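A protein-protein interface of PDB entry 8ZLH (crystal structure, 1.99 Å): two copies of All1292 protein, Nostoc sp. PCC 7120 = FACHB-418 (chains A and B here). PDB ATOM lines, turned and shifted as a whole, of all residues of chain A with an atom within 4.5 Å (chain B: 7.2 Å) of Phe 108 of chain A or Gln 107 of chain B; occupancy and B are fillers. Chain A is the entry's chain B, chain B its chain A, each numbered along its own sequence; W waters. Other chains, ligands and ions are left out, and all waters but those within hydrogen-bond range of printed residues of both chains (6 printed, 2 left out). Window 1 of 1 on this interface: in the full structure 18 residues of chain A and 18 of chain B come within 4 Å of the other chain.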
ATOM      1  N   VAL A  23      -6.636  -3.383  -5.402  1.00  0.00           N
ATOM      2  CA  VAL A  23      -6.866  -3.895  -6.753  1.00  0.00           C
ATOM      3  C   VAL A  23      -7.094  -5.398  -6.716  1.00  0.00           C
ATOM      4  O   VAL A  23      -8.059  -5.912  -7.300  1.00  0.00           O
ATOM      5  CB  VAL A  23      -5.693  -3.517  -7.672  1.00  0.00           C
ATOM      6  CG1 VAL A  23      -5.750  -4.284  -8.962  1.00  0.00           C
ATOM      7  CG2 VAL A  23      -5.743  -2.021  -7.956  1.00  0.00           C
ATOM      8  N   GLN A  27     -10.867  -6.814  -8.406  1.00  0.00           N
ATOM      9  CA  GLN A  27     -10.539  -6.902  -9.823  1.00  0.00           C
ATOM     10  C   GLN A  27     -11.785  -6.915 -10.702  1.00  0.00           C
ATOM     11  O   GLN A  27     -11.797  -6.311 -11.777  1.00  0.00           O
ATOM     12  CB  GLN A  27      -9.717  -8.161 -10.108  1.00  0.00           C
ATOM     13  CG  GLN A  27      -8.219  -7.962  -9.840  1.00  0.00           C
ATOM     14  CD  GLN A  27      -7.392  -9.143 -10.272  1.00  0.00           C
ATOM     15  OE1 GLN A  27      -7.911 -10.100 -10.888  1.00  0.00           O
ATOM     16  NE2 GLN A  27      -6.092  -9.083 -10.000  1.00  0.00           N
ATOM     17  N   LEU A  30     -13.378  -3.354 -10.738  1.00  0.00           N
ATOM     18  CA  LEU A  30     -12.489  -2.501 -11.522  1.00  0.00           C
ATOM     19  C   LEU A  30     -12.539  -2.867 -13.008  1.00  0.00           C
ATOM     20  O   LEU A  30     -12.499  -1.980 -13.867  1.00  0.00           O
ATOM     21  CB  LEU A  30     -11.052  -2.586 -10.976  1.00  0.00           C
ATOM     22  CG  LEU A  30     -10.760  -1.882  -9.629  1.00  0.00           C
ATOM     23  CD1 LEU A  30      -9.440  -2.356  -8.950  1.00  0.00           C
ATOM     24  CD2 LEU A  30     -10.736  -0.330  -9.760  1.00  0.00           C
ATOM     25  N   ALA A  31     -12.626  -4.168 -13.338  1.00  0.00           N
ATOM     26  CA  ALA A  31     -12.756  -4.554 -14.747  1.00  0.00           C
ATOM     27  C   ALA A  31     -14.073  -4.070 -15.351  1.00  0.00           C
ATOM     28  O   ALA A  31     -14.097  -3.540 -16.473  1.00  0.00           O
ATOM     29  CB  ALA A  31     -12.635  -6.074 -14.905  1.00  0.00           C
ATOM     30  N   GLU A  92      -7.671  -7.301 -20.854  1.00  0.00           N
ATOM     31  CA  GLU A  92      -6.874  -6.832 -19.700  1.00  0.00           C
ATOM     32  C   GLU A  92      -7.212  -5.397 -19.297  1.00  0.00           C
ATOM     33  O   GLU A  92      -7.495  -4.577 -20.173  1.00  0.00           O
ATOM     34  CB  GLU A  92      -5.393  -6.958 -20.024  1.00  0.00           C
ATOM     35  CG  GLU A  92      -5.049  -6.641 -21.455  1.00  0.00           C
ATOM     36  CD  GLU A  92      -3.555  -6.737 -21.648  1.00  0.00           C
ATOM     37  OE1 GLU A  92      -2.895  -7.094 -20.668  1.00  0.00           O
ATOM     38  OE2 GLU A  92      -3.071  -6.450 -22.751  1.00  0.00           O
ATOM     39  N   VAL A  93      -7.150  -5.140 -17.999  1.00  0.00           N
ATOM     40  CA  VAL A  93      -7.443  -3.798 -17.449  1.00  0.00           C
ATOM     41  C   VAL A  93      -6.141  -3.042 -17.229  1.00  0.00           C
ATOM     42  O   VAL A  93      -5.192  -3.640 -16.737  1.00  0.00           O
ATOM     43  CB  VAL A  93      -8.189  -3.925 -16.112  1.00  0.00           C
ATOM     44  CG1 VAL A  93      -8.359  -2.593 -15.401  1.00  0.00           C
ATOM     45  CG2 VAL A  93      -9.516  -4.642 -16.274  1.00  0.00           C
ATOM     46  N   ILE A 106      -1.324  -0.069 -12.829  1.00  0.00           N
ATOM     47  CA  ILE A 106      -2.305  -1.100 -12.524  1.00  0.00           C
ATOM     48  C   ILE A 106      -2.583  -1.835 -13.825  1.00  0.00           C
ATOM     49  O   ILE A 106      -3.007  -1.219 -14.813  1.00  0.00           O
ATOM     50  CB  ILE A 106      -3.592  -0.507 -11.930  1.00  0.00           C
ATOM     51  CG1 ILE A 106      -3.319   0.125 -10.567  1.00  0.00           C
ATOM     52  CG2 ILE A 106      -4.686  -1.535 -11.831  1.00  0.00           C
ATOM     53  CD1 ILE A 106      -4.347   1.129 -10.140  1.00  0.00           C
ATOM     54  N   GLN A 107      -2.302  -3.137 -13.843  1.00  0.00           N
ATOM     55  CA  GLN A 107      -2.564  -3.939 -15.030  1.00  0.00           C
ATOM     56  C   GLN A 107      -2.845  -5.375 -14.630  1.00  0.00           C
ATOM     57  O   GLN A 107      -2.054  -5.993 -13.911  1.00  0.00           O
ATOM     58  CB  GLN A 107      -1.391  -3.880 -16.016  1.00  0.00           C
ATOM     59  CG  GLN A 107      -1.840  -3.993 -17.482  1.00  0.00           C
ATOM     60  CD  GLN A 107      -0.718  -4.324 -18.455  1.00  0.00           C
ATOM     61  OE1 GLN A 107       0.401  -4.683 -18.055  1.00  0.00           O
ATOM     62  NE2 GLN A 107      -0.980  -4.094 -19.743  1.00  0.00           N
ATOM     63  N   PHE A 108      -3.964  -5.908 -15.105  1.00  0.00           N
ATOM     64  CA  PHE A 108      -4.268  -7.304 -14.827  1.00  0.00           C
ATOM     65  C   PHE A 108      -5.273  -7.814 -15.855  1.00  0.00           C
ATOM     66  O   PHE A 108      -6.159  -7.068 -16.292  1.00  0.00           O
ATOM     67  CB  PHE A 108      -4.788  -7.461 -13.390  1.00  0.00           C
ATOM     68  CG  PHE A 108      -6.033  -6.665 -13.106  1.00  0.00           C
ATOM     69  CD1 PHE A 108      -7.282  -7.211 -13.317  1.00  0.00           C
ATOM     70  CD2 PHE A 108      -5.950  -5.363 -12.614  1.00  0.00           C
ATOM     71  CE1 PHE A 108      -8.442  -6.473 -13.055  1.00  0.00           C
ATOM     72  CE2 PHE A 108      -7.107  -4.613 -12.362  1.00  0.00           C
ATOM     73  CZ  PHE A 108      -8.347  -5.168 -12.579  1.00  0.00           C
ATOM     74  N   ALA A 109      -5.104  -9.079 -16.258  1.00  0.00           N
ATOM     75  CA  ALA A 109      -6.018  -9.752 -17.168  1.00  0.00           C
ATOM     76  C   ALA A 109      -6.962 -10.596 -16.335  1.00  0.00           C
ATOM     77  O   ALA A 109      -6.570 -11.674 -15.874  1.00  0.00           O
ATOM     78  CB  ALA A 109      -5.250 -10.624 -18.163  1.00  0.00           C
ATOM     79  N   PRO A 110      -8.195 -10.162 -16.092  1.00  0.00           N
ATOM     80  CA  PRO A 110      -9.031 -10.821 -15.087  1.00  0.00           C
ATOM     81  C   PRO A 110      -9.732 -12.037 -15.676  1.00  0.00           C
ATOM     82  O   PRO A 110      -9.659 -12.317 -16.876  1.00  0.00           O
ATOM     83  CB  PRO A 110     -10.047  -9.741 -14.713  1.00  0.00           C
ATOM     84  CG  PRO A 110     -10.188  -8.920 -15.970  1.00  0.00           C
ATOM     85  CD  PRO A 110      -8.816  -8.938 -16.625  1.00  0.00           C
ATOM     86  N   ASP B  20      -7.202 -18.061 -11.670  1.00  0.00           N
ATOM     87  CA  ASP B  20      -7.301 -16.638 -11.373  1.00  0.00           C
ATOM     88  C   ASP B  20      -7.091 -16.381  -9.883  1.00  0.00           C
ATOM     89  O   ASP B  20      -6.363 -15.450  -9.498  1.00  0.00           O
ATOM     90  CB  ASP B  20      -8.656 -16.099 -11.846  1.00  0.00           C
ATOM     91  CG  ASP B  20      -8.806 -14.626 -11.577  1.00  0.00           C
ATOM     92  OD1 ASP B  20      -8.233 -13.824 -12.357  1.00  0.00           O
ATOM     93  OD2 ASP B  20      -9.490 -14.285 -10.593  1.00  0.00           O
ATOM     94  N   VAL B  23      -3.340 -16.892  -8.934  1.00  0.00           N
ATOM     95  CA  VAL B  23      -2.487 -15.778  -9.337  1.00  0.00           C
ATOM     96  C   VAL B  23      -2.666 -14.599  -8.385  1.00  0.00           C
ATOM     97  O   VAL B  23      -1.687 -14.089  -7.831  1.00  0.00           O
ATOM     98  CB  VAL B  23      -2.770 -15.412 -10.808  1.00  0.00           C
ATOM     99  CG1 VAL B  23      -2.076 -14.126 -11.217  1.00  0.00           C
ATOM    100  CG2 VAL B  23      -2.358 -16.586 -11.704  1.00  0.00           C
ATOM    101  N   LYS B  24      -3.925 -14.175  -8.148  1.00  0.00           N
ATOM    102  CA  LYS B  24      -4.189 -13.040  -7.257  1.00  0.00           C
ATOM    103  C   LYS B  24      -3.489 -13.196  -5.914  1.00  0.00           C
ATOM    104  O   LYS B  24      -2.960 -12.228  -5.361  1.00  0.00           O
ATOM    105  CB  LYS B  24      -5.689 -12.885  -6.987  1.00  0.00           C
ATOM    106  CG  LYS B  24      -6.535 -12.393  -8.104  1.00  0.00           C
ATOM    107  CD  LYS B  24      -7.925 -12.065  -7.558  1.00  0.00           C
ATOM    108  CE  LYS B  24      -9.012 -12.217  -8.601  1.00  0.00           C
ATOM    109  NZ  LYS B  24     -10.377 -12.534  -8.025  1.00  0.00           N
ATOM    110  N   GLN B  27       0.980 -13.208  -6.369  1.00  0.00           N
ATOM    111  CA  GLN B  27       1.577 -12.335  -7.375  1.00  0.00           C
ATOM    112  C   GLN B  27       3.073 -12.165  -7.147  1.00  0.00           C
ATOM    113  O   GLN B  27       3.853 -12.199  -8.106  1.00  0.00           O
ATOM    114  CB  GLN B  27       0.871 -10.974  -7.386  1.00  0.00           C
ATOM    115  CG  GLN B  27      -0.566 -11.050  -7.974  1.00  0.00           C
ATOM    116  CD  GLN B  27      -1.072  -9.708  -8.512  1.00  0.00           C
ATOM    117  OE1 GLN B  27      -0.371  -8.698  -8.465  1.00  0.00           O
ATOM    118  NE2 GLN B  27      -2.289  -9.694  -9.009  1.00  0.00           N
ATOM    119  N   ILE B  83       0.685  -9.133 -27.695  1.00  0.00           N
ATOM    120  CA  ILE B  83       0.839  -8.998 -26.247  1.00  0.00           C
ATOM    121  C   ILE B  83       2.148  -9.643 -25.804  1.00  0.00           C
ATOM    122  O   ILE B  83       2.881  -9.096 -24.975  1.00  0.00           O
ATOM    123  CB  ILE B  83      -0.357  -9.646 -25.525  1.00  0.00           C
ATOM    124  CG1 ILE B  83      -1.630  -8.834 -25.736  1.00  0.00           C
ATOM    125  CG2 ILE B  83      -0.069  -9.747 -24.028  1.00  0.00           C
ATOM    126  CD1 ILE B  83      -2.891  -9.589 -25.328  1.00  0.00           C
ATOM    127  N   ILE B  84       2.466 -10.818 -26.358  1.00  0.00           N
ATOM    128  CA  ILE B  84       3.707 -11.495 -25.976  1.00  0.00           C
ATOM    129  C   ILE B  84       4.919 -10.683 -26.416  1.00  0.00           C
ATOM    130  O   ILE B  84       5.821 -10.422 -25.615  1.00  0.00           O
ATOM    131  CB  ILE B  84       3.749 -12.936 -26.523  1.00  0.00           C
ATOM    132  CG1 ILE B  84       2.763 -13.827 -25.763  1.00  0.00           C
ATOM    133  CG2 ILE B  84       5.170 -13.516 -26.509  1.00  0.00           C
ATOM    134  CD1 ILE B  84       2.500 -15.133 -26.462  1.00  0.00           C
ATOM    135  N   HIS B  86       5.169  -7.511 -27.016  1.00  0.00           N
ATOM    136  CA  HIS B  86       5.291  -6.210 -26.372  1.00  0.00           C
ATOM    137  C   HIS B  86       5.503  -6.290 -24.866  1.00  0.00           C
ATOM    138  O   HIS B  86       5.731  -5.250 -24.248  1.00  0.00           O
ATOM    139  CB  HIS B  86       4.051  -5.347 -26.637  1.00  0.00           C
ATOM    140  CG  HIS B  86       3.780  -5.076 -28.091  1.00  0.00           C
ATOM    141  ND1 HIS B  86       2.509  -5.116 -28.628  1.00  0.00           N
ATOM    142  CD2 HIS B  86       4.610  -4.760 -29.114  1.00  0.00           C
ATOM    143  CE1 HIS B  86       2.568  -4.828 -29.918  1.00  0.00           C
ATOM    144  NE2 HIS B  86       3.833  -4.616 -30.239  1.00  0.00           N
ATOM    145  N   ASN B  87       5.419  -7.473 -24.255  1.00  0.00           N
ATOM    146  CA  ASN B  87       5.566  -7.555 -22.805  1.00  0.00           C
ATOM    147  C   ASN B  87       6.886  -6.932 -22.375  1.00  0.00           C
ATOM    148  O   ASN B  87       7.926  -7.144 -23.008  1.00  0.00           O
ATOM    149  CB  ASN B  87       5.502  -9.002 -22.305  1.00  0.00           C
ATOM    150  CG  ASN B  87       5.287  -9.073 -20.785  1.00  0.00           C
ATOM    151  OD1 ASN B  87       4.217  -8.691 -20.273  1.00  0.00           O
ATOM    152  ND2 ASN B  87       6.326  -9.491 -20.052  1.00  0.00           N
ATOM    153  N   GLN B  88       6.825  -6.152 -21.300  1.00  0.00           N
ATOM    154  CA  GLN B  88       7.972  -5.473 -20.701  1.00  0.00           C
ATOM    155  C   GLN B  88       8.271  -6.184 -19.392  1.00  0.00           C
ATOM    156  O   GLN B  88       7.667  -5.864 -18.349  1.00  0.00           O
ATOM    157  CB  GLN B  88       7.677  -3.989 -20.451  1.00  0.00           C
ATOM    158  CG  GLN B  88       7.412  -3.138 -21.664  1.00  0.00           C
ATOM    159  CD  GLN B  88       8.436  -3.317 -22.763  1.00  0.00           C
ATOM    160  OE1 GLN B  88       9.594  -2.936 -22.612  1.00  0.00           O
ATOM    161  NE2 GLN B  88       7.978  -3.751 -23.918  1.00  0.00           N
ATOM    162  N   GLU B  92       6.031  -6.163 -16.236  1.00  0.00           N
ATOM    163  CA  GLU B  92       4.844  -6.981 -16.444  1.00  0.00           C
ATOM    164  C   GLU B  92       5.214  -8.459 -16.410  1.00  0.00           C
ATOM    165  O   GLU B  92       6.109  -8.891 -17.144  1.00  0.00           O
ATOM    166  CB  GLU B  92       4.226  -6.681 -17.805  1.00  0.00           C
ATOM    167  CG  GLU B  92       3.611  -5.310 -17.952  1.00  0.00           C
ATOM    168  CD  GLU B  92       3.371  -5.032 -19.419  1.00  0.00           C
ATOM    169  OE1 GLU B  92       4.339  -5.110 -20.196  1.00  0.00           O
ATOM    170  OE2 GLU B  92       2.211  -4.809 -19.796  1.00  0.00           O
ATOM    171  N   VAL B  93       4.500  -9.223 -15.595  1.00  0.00           N
ATOM    172  CA  VAL B  93       4.538 -10.680 -15.649  1.00  0.00           C
ATOM    173  C   VAL B  93       3.609 -11.148 -16.760  1.00  0.00           C
ATOM    174  O   VAL B  93       2.455 -10.711 -16.832  1.00  0.00           O
ATOM    175  CB  VAL B  93       4.116 -11.284 -14.301  1.00  0.00           C
ATOM    176  CG1 VAL B  93       4.028 -12.842 -14.401  1.00  0.00           C
ATOM    177  CG2 VAL B  93       5.053 -10.837 -13.216  1.00  0.00           C
ATOM    178  N   LEU B  94       4.103 -12.049 -17.623  1.00  0.00           N
ATOM    179  CA  LEU B  94       3.278 -12.706 -18.642  1.00  0.00           C
ATOM    180  C   LEU B  94       3.482 -14.207 -18.580  1.00  0.00           C
ATOM    181  O   LEU B  94       4.626 -14.678 -18.652  1.00  0.00           O
ATOM    182  CB  LEU B  94       3.624 -12.254 -20.067  1.00  0.00           C
ATOM    183  CG  LEU B  94       2.658 -12.821 -21.115  1.00  0.00           C
ATOM    184  CD1 LEU B  94       2.288 -11.807 -22.135  1.00  0.00           C
ATOM    185  CD2 LEU B  94       3.158 -14.099 -21.821  1.00  0.00           C
ATOM    186  N   MET B  95       2.382 -14.955 -18.536  1.00  0.00           N
ATOM    187  CA  MET B  95       2.444 -16.412 -18.566  1.00  0.00           C
ATOM    188  C   MET B  95       1.179 -16.835 -19.300  1.00  0.00           C
ATOM    189  O   MET B  95       0.242 -16.047 -19.400  1.00  0.00           O
ATOM    190  CB  MET B  95       2.457 -16.946 -17.121  1.00  0.00           C
ATOM    191  CG  MET B  95       3.799 -16.959 -16.490  1.00  0.00           C
ATOM    192  SD  MET B  95       3.602 -17.487 -14.775  1.00  0.00           S
ATOM    193  CE  MET B  95       5.132 -16.884 -14.021  1.00  0.00           C
ATOM    194  N   ILE B  96       1.113 -18.078 -19.784  1.00  0.00           N
ATOM    195  CA  ILE B  96      -0.152 -18.622 -20.276  1.00  0.00           C
ATOM    196  C   ILE B  96      -0.457 -19.916 -19.533  1.00  0.00           C
ATOM    197  O   ILE B  96       0.351 -20.854 -19.541  1.00  0.00           O
ATOM    198  CB  ILE B  96      -0.174 -18.882 -21.797  1.00  0.00           C
ATOM    199  CG1 ILE B  96       1.009 -19.725 -22.266  1.00  0.00           C
ATOM    200  CG2 ILE B  96      -0.228 -17.544 -22.559  1.00  0.00           C
ATOM    201  CD1 ILE B  96       1.117 -19.816 -23.791  1.00  0.00           C
ATOM    202  N   LYS B 104      -5.144 -19.523 -21.314  1.00  0.00           N
ATOM    203  CA  LYS B 104      -5.650 -18.427 -20.497  1.00  0.00           C
ATOM    204  C   LYS B 104      -4.508 -17.446 -20.249  1.00  0.00           C
ATOM    205  O   LYS B 104      -3.475 -17.826 -19.680  1.00  0.00           O
ATOM    206  CB  LYS B 104      -6.238 -18.939 -19.179  1.00  0.00           C
ATOM    207  CG  LYS B 104      -6.220 -17.850 -18.095  1.00  0.00           C
ATOM    208  CD  LYS B 104      -7.518 -17.739 -17.326  1.00  0.00           C
ATOM    209  CE  LYS B 104      -7.382 -16.740 -16.197  1.00  0.00           C
ATOM    210  NZ  LYS B 104      -8.072 -15.491 -16.613  1.00  0.00           N
ATOM    211  N   LEU B 105      -4.685 -16.195 -20.676  1.00  0.00           N
ATOM    212  CA  LEU B 105      -3.623 -15.210 -20.509  1.00  0.00           C
ATOM    213  C   LEU B 105      -3.459 -14.801 -19.050  1.00  0.00           C
ATOM    214  O   LEU B 105      -4.415 -14.377 -18.399  1.00  0.00           O
ATOM    215  CB  LEU B 105      -3.881 -13.976 -21.371  1.00  0.00           C
ATOM    216  CG  LEU B 105      -2.836 -12.872 -21.156  1.00  0.00           C
ATOM    217  CD1 LEU B 105      -1.503 -13.257 -21.824  1.00  0.00           C
ATOM    218  CD2 LEU B 105      -3.313 -11.527 -21.647  1.00  0.00           C
ATOM    219  N   ILE B 106      -2.229 -14.868 -18.559  1.00  0.00           N
ATOM    220  CA  ILE B 106      -1.845 -14.301 -17.269  1.00  0.00           C
ATOM    221  C   ILE B 106      -0.929 -13.122 -17.558  1.00  0.00           C
ATOM    222  O   ILE B 106       0.181 -13.319 -18.066  1.00  0.00           O
ATOM    223  CB  ILE B 106      -1.132 -15.324 -16.379  1.00  0.00           C
ATOM    224  CG1 ILE B 106      -2.084 -16.461 -15.983  1.00  0.00           C
ATOM    225  CG2 ILE B 106      -0.538 -14.614 -15.155  1.00  0.00           C
ATOM    226  CD1 ILE B 106      -1.367 -17.748 -15.486  1.00  0.00           C
ATOM    227  N   GLN B 107      -1.387 -11.895 -17.250  1.00  0.00           N
ATOM    228  CA  GLN B 107      -0.555 -10.701 -17.360  1.00  0.00           C
ATOM    229  C   GLN B 107      -0.940  -9.747 -16.250  1.00  0.00           C
ATOM    230  O   GLN B 107      -2.132  -9.468 -16.070  1.00  0.00           O
ATOM    231  CB  GLN B 107      -0.703 -10.003 -18.722  1.00  0.00           C
ATOM    232  CG  GLN B 107       0.608  -9.305 -19.142  1.00  0.00           C
ATOM    233  CD  GLN B 107       0.502  -8.415 -20.371  1.00  0.00           C
ATOM    234  OE1 GLN B 107      -0.559  -8.246 -20.943  1.00  0.00           O
ATOM    235  NE2 GLN B 107       1.644  -8.005 -20.883  1.00  0.00           N
ATOM    236  N   PHE B 108       0.060  -9.246 -15.514  1.00  0.00           N
ATOM    237  CA  PHE B 108      -0.196  -8.333 -14.417  1.00  0.00           C
ATOM    238  C   PHE B 108       1.080  -7.583 -14.084  1.00  0.00           C
ATOM    239  O   PHE B 108       2.193  -8.102 -14.244  1.00  0.00           O
ATOM    240  CB  PHE B 108      -0.758  -9.037 -13.174  1.00  0.00           C
ATOM    241  CG  PHE B 108       0.171 -10.088 -12.578  1.00  0.00           C
ATOM    242  CD1 PHE B 108       1.185  -9.729 -11.687  1.00  0.00           C
ATOM    243  CD2 PHE B 108       0.006 -11.424 -12.895  1.00  0.00           C
ATOM    244  CE1 PHE B 108       2.020 -10.702 -11.144  1.00  0.00           C
ATOM    245  CE2 PHE B 108       0.853 -12.407 -12.370  1.00  0.00           C
ATOM    246  CZ  PHE B 108       1.856 -12.039 -11.490  1.00  0.00           C
ATOM    247  N   ALA B 109       0.903  -6.338 -13.656  1.00  0.00           N
ATOM    248  CA  ALA B 109       2.043  -5.548 -13.219  1.00  0.00           C
ATOM    249  C   ALA B 109       2.116  -5.630 -11.701  1.00  0.00           C
ATOM    250  O   ALA B 109       1.342  -4.954 -11.015  1.00  0.00           O
ATOM    251  CB  ALA B 109       1.895  -4.098 -13.676  1.00  0.00           C
HETATM  252  O   HOH W   1      -4.098  -7.506  -9.099  1.00  0.00           O
HETATM  253  O   HOH W   2      -1.210  -3.974 -11.315  1.00  0.00           O
HETATM  254  O   HOH W   3      -3.924 -10.811 -10.693  1.00  0.00           O
HETATM  255  O   HOH W   4     -10.279 -11.483 -11.734  1.00  0.00           O
HETATM  256  O   HOH W   5      -2.353  -6.740 -10.711  1.00  0.00           O
HETATM  257  O   HOH W   6      -3.806 -12.156 -15.365  1.00  0.00           O
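Of the 20 printed residues of chain B, 8 touch a printed residue of chain A.
Hydrophobic or aromatic side chains of chain B that line the printed part of chain A: Phe 108.
Of the 11 printed residues of chain A, 6 touch a printed residue of chain B.
Among the printed residues, no Asp or Glu carboxylate lies within 4 Å of a Lys or Arg side-chain nitrogen of the other chain.
Gln 27 of chain A touches its own counterpart, Gln 27 of chain B.
Glu 92 of chain A touches Gln 107 of chain B, and with the chains exchanged Gln 107 of chain A touches Glu 92 of chain B.
Gln 107 of chain A touches Phe 108 of chain B, and with the chains exchanged Phe 108 of chain A touches Gln 107 of chain B.
Gln 107 of chain A touches Ala 109 of chain B, and with the chains exchanged Ala 109 of chain A touches Gln 107 of chain B.
8 positions are printed for both chains.
The side-chain carboxylate (OE2) of Glu 92 of chain B lies close to the side-chain amide oxygen (OE1) of Gln 107 of chain A (2.5 Å).
The backbone carbonyl oxygen (O) of Gln 107 of chain A lies within hydrogen-bond range of the backbone NH (N) of Ala 109 of chain B, 3.0 Å away.
OE1 of Glu 92 of chain A sits close to OE1 of Gln 107 of chain B (2.6 Å).
The backbone carbonyl oxygen (O) of Gln 107 of chain B sits at hydrogen-bond distance from the backbone NH (N) of Ala 109 of chain A, at 3.0 Å.
Among the printed residues, merely in contact across the chains: Gln 27 of chain A with Lys 24 of chain B, Gln 27 of chain A with Gln 27 of chain B, Gln 107 of chain A with Phe 108 of chain B, Phe 108 of chain A with Gln 107 of chain B, Ala 109 of chain A with Leu 105 of chain B and Pro 110 of chain A with Lys 104 of chain B.
Water W3 bridges the side-chain amide nitrogen (NE2) of Gln 27 of chain B (2.6 Å) and the side-chain amide nitrogen (NE2) of Gln 27 of chain A (2.9 Å).
Water W1 lies within hydrogen-bond range of NE2 of Gln 27 of chain A (2.7 Å) and NE2 of Gln 27 of chain B (2.8 Å).
Water W2 lies within hydrogen-bond range of the backbone carbonyl oxygen (O) of Ala 109 of chain B (2.8 Å) and the backbone NH (N) of Gln 107 of chain A (2.9 Å).
Water W6 lies within hydrogen-bond range of O of Ala 109 of chain A (2.9 Å) and N of Gln 107 of chain B (3.1 Å).
Water W4 lies within hydrogen-bond range of OE1 of Gln 27 of chain A and OD2 of Asp 20 of chain B.
Water W5 lies within hydrogen-bond range of the backbone carbonyl oxygen (O) of Gln 107 of chain A (3.3 Å) and the side-chain amide nitrogen (NE2) of Gln 27 of chain B (3.4 Å).
OD2 of Asp 20 of chain B lies within salt-bridge range of NZ of Lys 24 of chain B (3.2 Å).
NE2 of Gln 107 of chain B sits at hydrogen-bond distance from OD1 of Asn 87 of chain B.
The backbone carbonyl oxygen (O) of Glu 92 of chain B is in hydrogen-bond range of the side-chain amide nitrogen (ND2) of Asn 87 of chain B (3.0 Å).
N of Gln 88 of chain B lies within hydrogen-bond range of OE1 of Glu 92 of chain B, 2.9 Å away.
OE2 of Glu 92 of chain B lies within hydrogen-bond range of NE2 of Gln 107 of chain B.
The backbone NH of Val 93 of chain A is in hydrogen-bond range of the backbone carbonyl oxygen of Phe 108 of chain A, at 2.8 Å.
Printed residues of chain B within 4 Å of Gln 107 of chain A: Glu 92, Phe 108 and Ala 109.
Phe 108 of chain A touches one residue of chain B.
Printed residues of chain A within 4 Å of Lys 104 of chain B: Pro 110.
Of the printed residues of chain A, Leu 105 of chain B touches Ala 109.
Gln 107 of chain B touches just these residues of chain A: Glu 92, Phe 108 and Ala 109.
Of the printed residues of chain A, Ala 109 of chain B touches Gln 107 (3.0 Å).
The nearest residue of chain A that does not touch Gln 107 of chain B is Gln 107 of chain A (4.1 Å).
The nearest printed residue of chain B that does not touch Gln 107 of chain A is Gln 107 of chain B (4.1 Å).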
